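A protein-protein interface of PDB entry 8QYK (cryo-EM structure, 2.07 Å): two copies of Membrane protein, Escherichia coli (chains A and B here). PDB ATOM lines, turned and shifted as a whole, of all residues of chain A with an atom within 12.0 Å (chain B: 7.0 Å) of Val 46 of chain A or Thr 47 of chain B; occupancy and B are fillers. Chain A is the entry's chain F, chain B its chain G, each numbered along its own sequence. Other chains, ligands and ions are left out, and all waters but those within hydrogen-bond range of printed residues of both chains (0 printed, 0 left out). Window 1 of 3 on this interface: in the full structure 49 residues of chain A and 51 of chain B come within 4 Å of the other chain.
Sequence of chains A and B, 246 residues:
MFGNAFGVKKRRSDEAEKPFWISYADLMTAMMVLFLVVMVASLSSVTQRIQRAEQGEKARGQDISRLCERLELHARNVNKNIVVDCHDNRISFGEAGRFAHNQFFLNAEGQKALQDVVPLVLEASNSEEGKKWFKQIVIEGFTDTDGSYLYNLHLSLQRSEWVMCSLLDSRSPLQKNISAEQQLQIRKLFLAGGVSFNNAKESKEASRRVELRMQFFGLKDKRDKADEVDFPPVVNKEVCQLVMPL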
ATOM      1  N   VAL A  37      -0.322 -16.475  -8.392  1.00  0.00           N
ATOM      2  CA  VAL A  37      -1.378 -17.436  -8.093  1.00  0.00           C
ATOM      3  C   VAL A  37      -2.514 -16.758  -7.340  1.00  0.00           C
ATOM      4  O   VAL A  37      -3.693 -16.981  -7.634  1.00  0.00           O
ATOM      5  CB  VAL A  37      -0.806 -18.629  -7.303  1.00  0.00           C
ATOM      6  CG1 VAL A  37      -1.916 -19.386  -6.594  1.00  0.00           C
ATOM      7  CG2 VAL A  37      -0.029 -19.555  -8.227  1.00  0.00           C
ATOM      8  N   VAL A  38      -2.176 -15.921  -6.360  1.00  0.00           N
ATOM      9  CA  VAL A  38      -3.197 -15.208  -5.606  1.00  0.00           C
ATOM     10  C   VAL A  38      -3.973 -14.272  -6.520  1.00  0.00           C
ATOM     11  O   VAL A  38      -5.193 -14.153  -6.406  1.00  0.00           O
ATOM     12  CB  VAL A  38      -2.563 -14.465  -4.415  1.00  0.00           C
ATOM     13  CG1 VAL A  38      -3.520 -13.430  -3.851  1.00  0.00           C
ATOM     14  CG2 VAL A  38      -2.158 -15.455  -3.332  1.00  0.00           C
ATOM     15  N   MET A  39      -3.289 -13.620  -7.463  1.00  0.00           N
ATOM     16  CA  MET A  39      -3.969 -12.728  -8.394  1.00  0.00           C
ATOM     17  C   MET A  39      -4.979 -13.482  -9.251  1.00  0.00           C
ATOM     18  O   MET A  39      -6.150 -13.094  -9.327  1.00  0.00           O
ATOM     19  CB  MET A  39      -2.940 -12.001  -9.262  1.00  0.00           C
ATOM     20  CG  MET A  39      -3.537 -11.164 -10.380  1.00  0.00           C
ATOM     21  SD  MET A  39      -2.411 -10.916 -11.765  1.00  0.00           S
ATOM     22  CE  MET A  39      -2.578 -12.463 -12.637  1.00  0.00           C
ATOM     23  N   VAL A  40      -4.551 -14.575  -9.894  1.00  0.00           N
ATOM     24  CA  VAL A  40      -5.481 -15.302 -10.759  1.00  0.00           C
ATOM     25  C   VAL A  40      -6.623 -15.900  -9.941  1.00  0.00           C
ATOM     26  O   VAL A  40      -7.796 -15.802 -10.327  1.00  0.00           O
ATOM     27  CB  VAL A  40      -4.754 -16.377 -11.598  1.00  0.00           C
ATOM     28  CG1 VAL A  40      -3.832 -15.733 -12.610  1.00  0.00           C
ATOM     29  CG2 VAL A  40      -3.982 -17.351 -10.729  1.00  0.00           C
ATOM     30  N   ALA A  41      -6.309 -16.502  -8.791  1.00  0.00           N
ATOM     31  CA  ALA A  41      -7.338 -17.137  -7.978  1.00  0.00           C
ATOM     32  C   ALA A  41      -8.328 -16.117  -7.433  1.00  0.00           C
ATOM     33  O   ALA A  41      -9.537 -16.361  -7.428  1.00  0.00           O
ATOM     34  CB  ALA A  41      -6.691 -17.924  -6.839  1.00  0.00           C
ATOM     35  N   SER A  42      -7.833 -14.967  -6.969  1.00  0.00           N
ATOM     36  CA  SER A  42      -8.705 -13.932  -6.432  1.00  0.00           C
ATOM     37  C   SER A  42      -9.574 -13.319  -7.519  1.00  0.00           C
ATOM     38  O   SER A  42     -10.759 -13.056  -7.292  1.00  0.00           O
ATOM     39  CB  SER A  42      -7.869 -12.851  -5.748  1.00  0.00           C
ATOM     40  OG  SER A  42      -7.352 -13.310  -4.514  1.00  0.00           O
ATOM     41  N   LEU A  43      -9.005 -13.071  -8.700  1.00  0.00           N
ATOM     42  CA  LEU A  43      -9.806 -12.549  -9.800  1.00  0.00           C
ATOM     43  C   LEU A  43     -10.920 -13.522 -10.157  1.00  0.00           C
ATOM     44  O   LEU A  43     -12.084 -13.128 -10.301  1.00  0.00           O
ATOM     45  CB  LEU A  43      -8.913 -12.270 -11.007  1.00  0.00           C
ATOM     46  CG  LEU A  43      -9.418 -11.246 -12.023  1.00  0.00           C
ATOM     47  CD1 LEU A  43      -9.976 -10.023 -11.313  1.00  0.00           C
ATOM     48  CD2 LEU A  43      -8.296 -10.854 -12.964  1.00  0.00           C
ATOM     49  N   SER A  44     -10.582 -14.811 -10.255  1.00  0.00           N
ATOM     50  CA  SER A  44     -11.589 -15.826 -10.540  1.00  0.00           C
ATOM     51  C   SER A  44     -12.665 -15.860  -9.462  1.00  0.00           C
ATOM     52  O   SER A  44     -13.862 -15.867  -9.770  1.00  0.00           O
ATOM     53  CB  SER A  44     -10.917 -17.193 -10.670  1.00  0.00           C
ATOM     54  OG  SER A  44     -11.868 -18.219 -10.884  1.00  0.00           O
ATOM     55  N   SER A  45     -12.257 -15.871  -8.193  1.00  0.00           N
ATOM     56  CA  SER A  45     -13.209 -15.997  -7.097  1.00  0.00           C
ATOM     57  C   SER A  45     -14.142 -14.792  -7.026  1.00  0.00           C
ATOM     58  O   SER A  45     -15.351 -14.944  -6.827  1.00  0.00           O
ATOM     59  CB  SER A  45     -12.456 -16.182  -5.780  1.00  0.00           C
ATOM     60  OG  SER A  45     -13.335 -16.108  -4.673  1.00  0.00           O
ATOM     61  N   VAL A  46     -13.601 -13.586  -7.203  1.00  0.00           N
ATOM     62  CA  VAL A  46     -14.431 -12.387  -7.124  1.00  0.00           C
ATOM     63  C   VAL A  46     -15.381 -12.309  -8.313  1.00  0.00           C
ATOM     64  O   VAL A  46     -16.555 -11.940  -8.165  1.00  0.00           O
ATOM     65  CB  VAL A  46     -13.540 -11.136  -7.010  1.00  0.00           C
ATOM     66  CG1 VAL A  46     -14.374  -9.876  -7.104  1.00  0.00           C
ATOM     67  CG2 VAL A  46     -12.774 -11.165  -5.701  1.00  0.00           C
ATOM     68  N   THR A  47     -14.899 -12.658  -9.510  1.00  0.00           N
ATOM     69  CA  THR A  47     -15.780 -12.684 -10.671  1.00  0.00           C
ATOM     70  C   THR A  47     -16.905 -13.692 -10.481  1.00  0.00           C
ATOM     71  O   THR A  47     -18.063 -13.415 -10.819  1.00  0.00           O
ATOM     72  CB  THR A  47     -14.976 -13.004 -11.930  1.00  0.00           C
ATOM     73  OG1 THR A  47     -13.975 -11.998 -12.123  1.00  0.00           O
ATOM     74  CG2 THR A  47     -15.882 -13.052 -13.149  1.00  0.00           C
ATOM     75  N   GLN A  48     -16.589 -14.863  -9.924  1.00  0.00           N
ATOM     76  CA  GLN A  48     -17.619 -15.869  -9.702  1.00  0.00           C
ATOM     77  C   GLN A  48     -18.591 -15.441  -8.607  1.00  0.00           C
ATOM     78  O   GLN A  48     -19.778 -15.763  -8.678  1.00  0.00           O
ATOM     79  CB  GLN A  48     -16.975 -17.217  -9.381  1.00  0.00           C
ATOM     80  CG  GLN A  48     -16.212 -17.797 -10.562  1.00  0.00           C
ATOM     81  CD  GLN A  48     -15.552 -19.123 -10.254  1.00  0.00           C
ATOM     82  OE1 GLN A  48     -15.598 -19.605  -9.127  1.00  0.00           O
ATOM     83  NE2 GLN A  48     -14.929 -19.720 -11.262  1.00  0.00           N
ATOM     84  N   ARG A  49     -18.171 -14.660  -7.622  1.00  0.00           N
ATOM     85  CA  ARG A  49     -19.104 -14.151  -6.586  1.00  0.00           C
ATOM     86  C   ARG A  49     -19.991 -13.048  -7.145  1.00  0.00           C
ATOM     87  O   ARG A  49     -21.090 -12.921  -6.679  1.00  0.00           O
ATOM     88  CB  ARG A  49     -18.355 -13.628  -5.366  1.00  0.00           C
ATOM     89  CG  ARG A  49     -17.678 -14.737  -4.581  1.00  0.00           C
ATOM     90  CD  ARG A  49     -16.894 -14.233  -3.402  1.00  0.00           C
ATOM     91  NE  ARG A  49     -17.124 -15.138  -2.293  1.00  0.00           N
ATOM     92  CZ  ARG A  49     -16.280 -16.074  -1.887  1.00  0.00           C
ATOM     93  NH1 ARG A  49     -15.029 -16.067  -2.302  1.00  0.00           N
ATOM     94  NH2 ARG A  49     -16.691 -16.996  -1.039  1.00  0.00           N
ATOM     95  N   ILE A  50     -19.501 -12.257  -8.076  1.00  0.00           N
ATOM     96  CA  ILE A  50     -20.365 -11.275  -8.728  1.00  0.00           C
ATOM     97  C   ILE A  50     -21.380 -11.977  -9.624  1.00  0.00           C
ATOM     98  O   ILE A  50     -22.579 -11.668  -9.601  1.00  0.00           O
ATOM     99  CB  ILE A  50     -19.521 -10.256  -9.515  1.00  0.00           C
ATOM    100  CG1 ILE A  50     -18.704  -9.390  -8.556  1.00  0.00           C
ATOM    101  CG2 ILE A  50     -20.407  -9.386 -10.384  1.00  0.00           C
ATOM    102  CD1 ILE A  50     -17.679  -8.519  -9.246  1.00  0.00           C
ATOM    103  N   GLN A  51     -20.914 -12.942 -10.420  1.00  0.00           N
ATOM    104  CA  GLN A  51     -21.818 -13.661 -11.309  1.00  0.00           C
ATOM    105  C   GLN A  51     -22.830 -14.494 -10.534  1.00  0.00           C
ATOM    106  O   GLN A  51     -23.984 -14.599 -10.954  1.00  0.00           O
ATOM    107  CB  GLN A  51     -21.023 -14.537 -12.274  1.00  0.00           C
ATOM    108  CG  GLN A  51     -20.183 -13.740 -13.261  1.00  0.00           C
ATOM    109  CD  GLN A  51     -19.383 -14.617 -14.200  1.00  0.00           C
ATOM    110  OE1 GLN A  51     -19.392 -15.842 -14.086  1.00  0.00           O
ATOM    111  NE2 GLN A  51     -18.682 -13.991 -15.138  1.00  0.00           N
ATOM    112  N   ARG A  52     -22.482 -15.072  -9.390  1.00  0.00           N
ATOM    113  CA  ARG A  52     -23.408 -15.884  -8.543  1.00  0.00           C
ATOM    114  C   ARG A  52     -24.471 -14.975  -7.941  1.00  0.00           C
ATOM    115  O   ARG A  52     -25.605 -15.423  -7.806  1.00  0.00           O
ATOM    116  CB  ARG A  52     -22.629 -16.613  -7.440  1.00  0.00           C
ATOM    117  CG  ARG A  52     -23.379 -16.940  -6.161  1.00  0.00           C
ATOM    118  CD  ARG A  52     -22.787 -18.160  -5.475  1.00  0.00           C
ATOM    119  NE  ARG A  52     -21.333 -18.187  -5.359  1.00  0.00           N
ATOM    120  CZ  ARG A  52     -20.660 -18.621  -4.301  1.00  0.00           C
ATOM    121  NH1 ARG A  52     -20.626 -17.905  -3.194  1.00  0.00           N
ATOM    122  NH2 ARG A  52     -19.995 -19.758  -4.365  1.00  0.00           N
ATOM    123  N   ALA A  53     -24.100 -13.749  -7.568  1.00  0.00           N
ATOM    124  CA  ALA A  53     -25.115 -12.812  -7.094  1.00  0.00           C
ATOM    125  C   ALA A  53     -26.049 -12.385  -8.224  1.00  0.00           C
ATOM    126  O   ALA A  53     -27.273 -12.313  -8.041  1.00  0.00           O
ATOM    127  CB  ALA A  53     -24.449 -11.596  -6.455  1.00  0.00           C
ATOM    128  N   GLU A  54     -25.487 -12.101  -9.404  1.00  0.00           N
ATOM    129  CA  GLU A  54     -26.312 -11.706 -10.542  1.00  0.00           C
ATOM    130  C   GLU A  54     -27.282 -12.816 -10.934  1.00  0.00           C
ATOM    131  O   GLU A  54     -28.465 -12.563 -11.193  1.00  0.00           O
ATOM    132  CB  GLU A  54     -25.425 -11.325 -11.727  1.00  0.00           C
ATOM    133  CG  GLU A  54     -24.802  -9.945 -11.631  1.00  0.00           C
ATOM    134  CD  GLU A  54     -23.745  -9.710 -12.694  1.00  0.00           C
ATOM    135  OE1 GLU A  54     -23.378 -10.678 -13.392  1.00  0.00           O
ATOM    136  OE2 GLU A  54     -23.283  -8.558 -12.834  1.00  0.00           O
ATOM    137  N   GLN A  55     -26.795 -14.059 -10.987  1.00  0.00           N
ATOM    138  CA  GLN A  55     -27.660 -15.179 -11.341  1.00  0.00           C
ATOM    139  C   GLN A  55     -28.702 -15.448 -10.267  1.00  0.00           C
ATOM    140  O   GLN A  55     -29.815 -15.867 -10.588  1.00  0.00           O
ATOM    141  CB  GLN A  55     -26.835 -16.440 -11.603  1.00  0.00           C
ATOM    142  CG  GLN A  55     -25.796 -16.297 -12.703  1.00  0.00           C
ATOM    143  CD  GLN A  55     -26.380 -16.444 -14.095  1.00  0.00           C
ATOM    144  OE1 GLN A  55     -27.598 -16.479 -14.273  1.00  0.00           O
ATOM    145  NE2 GLN A  55     -25.508 -16.532 -15.092  1.00  0.00           N
ATOM    146  N   ALA B  41      -5.369  -3.480  -9.399  1.00  0.00           N
ATOM    147  CA  ALA B  41      -6.094  -2.799 -10.465  1.00  0.00           C
ATOM    148  C   ALA B  41      -7.287  -3.616 -10.946  1.00  0.00           C
ATOM    149  O   ALA B  41      -8.385  -3.076 -11.131  1.00  0.00           O
ATOM    150  CB  ALA B  41      -5.146  -2.503 -11.627  1.00  0.00           C
ATOM    151  N   SER B  42      -7.093  -4.921 -11.147  1.00  0.00           N
ATOM    152  CA  SER B  42      -8.165  -5.771 -11.648  1.00  0.00           C
ATOM    153  C   SER B  42      -9.302  -5.882 -10.643  1.00  0.00           C
ATOM    154  O   SER B  42     -10.475  -5.823 -11.022  1.00  0.00           O
ATOM    155  CB  SER B  42      -7.614  -7.155 -11.986  1.00  0.00           C
ATOM    156  OG  SER B  42      -6.414  -7.053 -12.726  1.00  0.00           O
ATOM    157  N   LEU B  43      -8.973  -6.052  -9.361  1.00  0.00           N
ATOM    158  CA  LEU B  43     -10.001  -6.133  -8.329  1.00  0.00           C
ATOM    159  C   LEU B  43     -10.750  -4.817  -8.191  1.00  0.00           C
ATOM    160  O   LEU B  43     -11.973  -4.810  -8.015  1.00  0.00           O
ATOM    161  CB  LEU B  43      -9.372  -6.536  -6.996  1.00  0.00           C
ATOM    162  CG  LEU B  43      -8.944  -7.999  -6.881  1.00  0.00           C
ATOM    163  CD1 LEU B  43      -8.257  -8.258  -5.554  1.00  0.00           C
ATOM    164  CD2 LEU B  43     -10.147  -8.910  -7.056  1.00  0.00           C
ATOM    165  N   SER B  44     -10.036  -3.692  -8.265  1.00  0.00           N
ATOM    166  CA  SER B  44     -10.696  -2.395  -8.236  1.00  0.00           C
ATOM    167  C   SER B  44     -11.622  -2.200  -9.425  1.00  0.00           C
ATOM    168  O   SER B  44     -12.692  -1.605  -9.271  1.00  0.00           O
ATOM    169  CB  SER B  44      -9.655  -1.279  -8.199  1.00  0.00           C
ATOM    170  OG  SER B  44      -8.744  -1.472  -7.135  1.00  0.00           O
ATOM    171  N   SER B  45     -11.234  -2.686 -10.603  1.00  0.00           N
ATOM    172  CA  SER B  45     -12.073  -2.520 -11.785  1.00  0.00           C
ATOM    173  C   SER B  45     -13.291  -3.438 -11.763  1.00  0.00           C
ATOM    174  O   SER B  45     -14.391  -3.012 -12.127  1.00  0.00           O
ATOM    175  CB  SER B  45     -11.248  -2.766 -13.045  1.00  0.00           C
ATOM    176  OG  SER B  45     -10.224  -1.800 -13.178  1.00  0.00           O
ATOM    177  N   VAL B  46     -13.127  -4.699 -11.352  1.00  0.00           N
ATOM    178  CA  VAL B  46     -14.260  -5.620 -11.400  1.00  0.00           C
ATOM    179  C   VAL B  46     -15.282  -5.280 -10.324  1.00  0.00           C
ATOM    180  O   VAL B  46     -16.460  -5.628 -10.448  1.00  0.00           O
ATOM    181  CB  VAL B  46     -13.797  -7.085 -11.285  1.00  0.00           C
ATOM    182  CG1 VAL B  46     -12.959  -7.476 -12.489  1.00  0.00           C
ATOM    183  CG2 VAL B  46     -13.045  -7.322  -9.989  1.00  0.00           C
ATOM    184  N   THR B  47     -14.860  -4.607  -9.257  1.00  0.00           N
ATOM    185  CA  THR B  47     -15.753  -4.230  -8.173  1.00  0.00           C
ATOM    186  C   THR B  47     -16.066  -2.740  -8.147  1.00  0.00           C
ATOM    187  O   THR B  47     -16.633  -2.262  -7.162  1.00  0.00           O
ATOM    188  CB  THR B  47     -15.163  -4.656  -6.824  1.00  0.00           C
ATOM    189  OG1 THR B  47     -14.016  -3.851  -6.525  1.00  0.00           O
ATOM    190  CG2 THR B  47     -14.763  -6.117  -6.848  1.00  0.00           C
ATOM    191  N   GLN B  48     -15.724  -1.996  -9.204  1.00  0.00           N
ATOM    192  CA  GLN B  48     -15.957  -0.553  -9.180  1.00  0.00           C
ATOM    193  C   GLN B  48     -17.442  -0.220  -9.142  1.00  0.00           C
ATOM    194  O   GLN B  48     -17.840   0.730  -8.462  1.00  0.00           O
ATOM    195  CB  GLN B  48     -15.289   0.131 -10.375  1.00  0.00           C
ATOM    196  CG  GLN B  48     -15.827  -0.258 -11.740  1.00  0.00           C
ATOM    197  CD  GLN B  48     -15.104   0.448 -12.872  1.00  0.00           C
ATOM    198  OE1 GLN B  48     -13.907   0.251 -13.078  1.00  0.00           O
ATOM    199  NE2 GLN B  48     -15.830   1.276 -13.612  1.00  0.00           N
ATOM    200  N   ARG B  49     -18.275  -0.973  -9.865  1.00  0.00           N
ATOM    201  CA  ARG B  49     -19.717  -0.769  -9.768  1.00  0.00           C
ATOM    202  C   ARG B  49     -20.214  -1.088  -8.365  1.00  0.00           C
ATOM    203  O   ARG B  49     -21.023  -0.343  -7.797  1.00  0.00           O
ATOM    204  CB  ARG B  49     -20.439  -1.625 -10.807  1.00  0.00           C
ATOM    205  CG  ARG B  49     -20.501  -1.001 -12.193  1.00  0.00           C
ATOM    206  CD  ARG B  49     -20.596  -2.062 -13.276  1.00  0.00           C
ATOM    207  NE  ARG B  49     -20.202  -1.548 -14.582  1.00  0.00           N
ATOM    208  CZ  ARG B  49     -20.021  -2.298 -15.660  1.00  0.00           C
ATOM    209  NH1 ARG B  49     -20.184  -3.609 -15.624  1.00  0.00           N
ATOM    210  NH2 ARG B  49     -19.666  -1.717 -16.802  1.00  0.00           N
ATOM    211  N   ILE B  50     -19.724  -2.184  -7.784  1.00  0.00           N
ATOM    212  CA  ILE B  50     -20.080  -2.528  -6.413  1.00  0.00           C
ATOM    213  C   ILE B  50     -19.594  -1.457  -5.448  1.00  0.00           C
ATOM    214  O   ILE B  50     -20.301  -1.092  -4.503  1.00  0.00           O
ATOM    215  CB  ILE B  50     -19.522  -3.916  -6.049  1.00  0.00           C
ATOM    216  CG1 ILE B  50     -20.072  -4.976  -7.004  1.00  0.00           C
ATOM    217  CG2 ILE B  50     -19.842  -4.263  -4.605  1.00  0.00           C
ATOM    218  CD1 ILE B  50     -19.596  -6.369  -6.696  1.00  0.00           C
ATOM    219  N   GLN B  51     -18.380  -0.941  -5.659  1.00  0.00           N
ATOM    220  CA  GLN B  51     -17.858   0.096  -4.774  1.00  0.00           C
ATOM    221  C   GLN B  51     -18.677   1.377  -4.867  1.00  0.00           C
ATOM    222  O   GLN B  51     -18.951   2.015  -3.847  1.00  0.00           O
ATOM    223  CB  GLN B  51     -16.386   0.374  -5.083  1.00  0.00           C
ATOM    224  CG  GLN B  51     -15.451  -0.763  -4.711  1.00  0.00           C
ATOM    225  CD  GLN B  51     -14.042  -0.557  -5.225  1.00  0.00           C
ATOM    226  OE1 GLN B  51     -13.770   0.388  -5.966  1.00  0.00           O
ATOM    227  NE2 GLN B  51     -13.134  -1.444  -4.835  1.00  0.00           N
ATOM    228  N   ARG B  52     -19.073   1.774  -6.078  1.00  0.00           N
ATOM    229  CA  ARG B  52     -19.908   2.964  -6.218  1.00  0.00           C
ATOM    230  C   ARG B  52     -21.273   2.764  -5.575  1.00  0.00           C
ATOM    231  O   ARG B  52     -21.789   3.669  -4.911  1.00  0.00           O
ATOM    232  CB  ARG B  52     -20.067   3.347  -7.688  1.00  0.00           C
ATOM    233  CG  ARG B  52     -18.847   4.002  -8.301  1.00  0.00           C
ATOM    234  CD  ARG B  52     -19.209   4.729  -9.587  1.00  0.00           C
ATOM    235  NE  ARG B  52     -19.670   3.818 -10.628  1.00  0.00           N
ATOM    236  CZ  ARG B  52     -18.877   3.226 -11.510  1.00  0.00           C
ATOM    237  NH1 ARG B  52     -17.567   3.417 -11.502  1.00  0.00           N
ATOM    238  NH2 ARG B  52     -19.411   2.423 -12.426  1.00  0.00           N
ATOM    239  N   ALA B  53     -21.875   1.586  -5.763  1.00  0.00           N
ATOM    240  CA  ALA B  53     -23.162   1.314  -5.132  1.00  0.00           C
ATOM    241  C   ALA B  53     -23.047   1.329  -3.614  1.00  0.00           C
ATOM    242  O   ALA B  53     -23.920   1.864  -2.922  1.00  0.00           O
ATOM    243  CB  ALA B  53     -23.713  -0.027  -5.618  1.00  0.00           C
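Val 46 of chain A touches Leu 43 of chain B, but with the chains exchanged Leu 43 of chain A does not touch Val 46 of chain B (4.1 Å).
Val 46 of chain A touches Thr 47 of chain B, but with the chains exchanged Thr 47 of chain A does not touch Val 46 of chain B (4.6 Å).
Ile 50 of chain A touches Val 46 of chain B, but with the chains exchanged Val 46 of chain A does not touch Ile 50 of chain B (6.3 Å).
Ile 50 of chain A touches its own counterpart, Ile 50 of chain B.
13 positions are printed for both chains.
Among the printed residues, pairs that only touch across the chains: Ile 50 of chain A with Val 46 of chain B (3.4 Å), Ile 50 of chain A with Ile 50 of chain B (3.7 Å), Val 46 of chain A with Leu 43 of chain B (3.7 Å), Leu 43 of chain A with Ser 42 of chain B (3.8 Å) and Val 46 of chain A with Thr 47 of chain B (3.8 Å).
Along chain B the printed residues that touch a printed residue of chain A span positions 42 to 50.
Hydrophobic or aromatic side chains of chain A within 4 Å of the printed part of chain B: Leu 43, Val 46 and Ile 50.
Among the printed residues, 5 pairs touch across the chains.
Of the printed residues of chain B, Leu 43 of chain A touches Ser 42.
Val 46 of chain A touches two residues of chain B.
Gln 48 of chain A touches none of the printed residues of chain B.
Of the printed residues of chain B, Ile 50 of chain A touches Val 46 (3.4 Å) and Ile 50 (3.7 Å).
Ala 53 of chain A touches none of the printed residues of chain B.
Of the printed residues of chain A, Ser 42 of chain B touches Leu 43.
No residue of chain A comes within 4 Å of Ser 44 of chain B.
No residue of chain A comes within 4 Å of Ser 45 of chain B.
Val 46 of chain B touches just one residue of chain A: Ile 50.
Thr 47 of chain B touches just one residue of chain A: Val 46.
No residue of chain A comes within 4 Å of Gln 48 of chain B.
Gln 51 of chain B touches none of the printed residues of chain A.
The nearest residue of chain B that does not touch Val 46 of chain A is Val 46 of chain B (4.1 Å).
O of Leu 43 of chain A is in hydrogen-bond range of OG1 of Thr 47 of chain A, at 2.9 Å.
The backbone carbonyl oxygen (O) of Leu 43 of chain B lies within hydrogen-bond range of the side-chain hydroxyl (OG1) of Thr 47 of chain B (2.7 Å).
OG1 of Thr 47 of chain B is in hydrogen-bond range of NE2 of Gln 51 of chain B.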
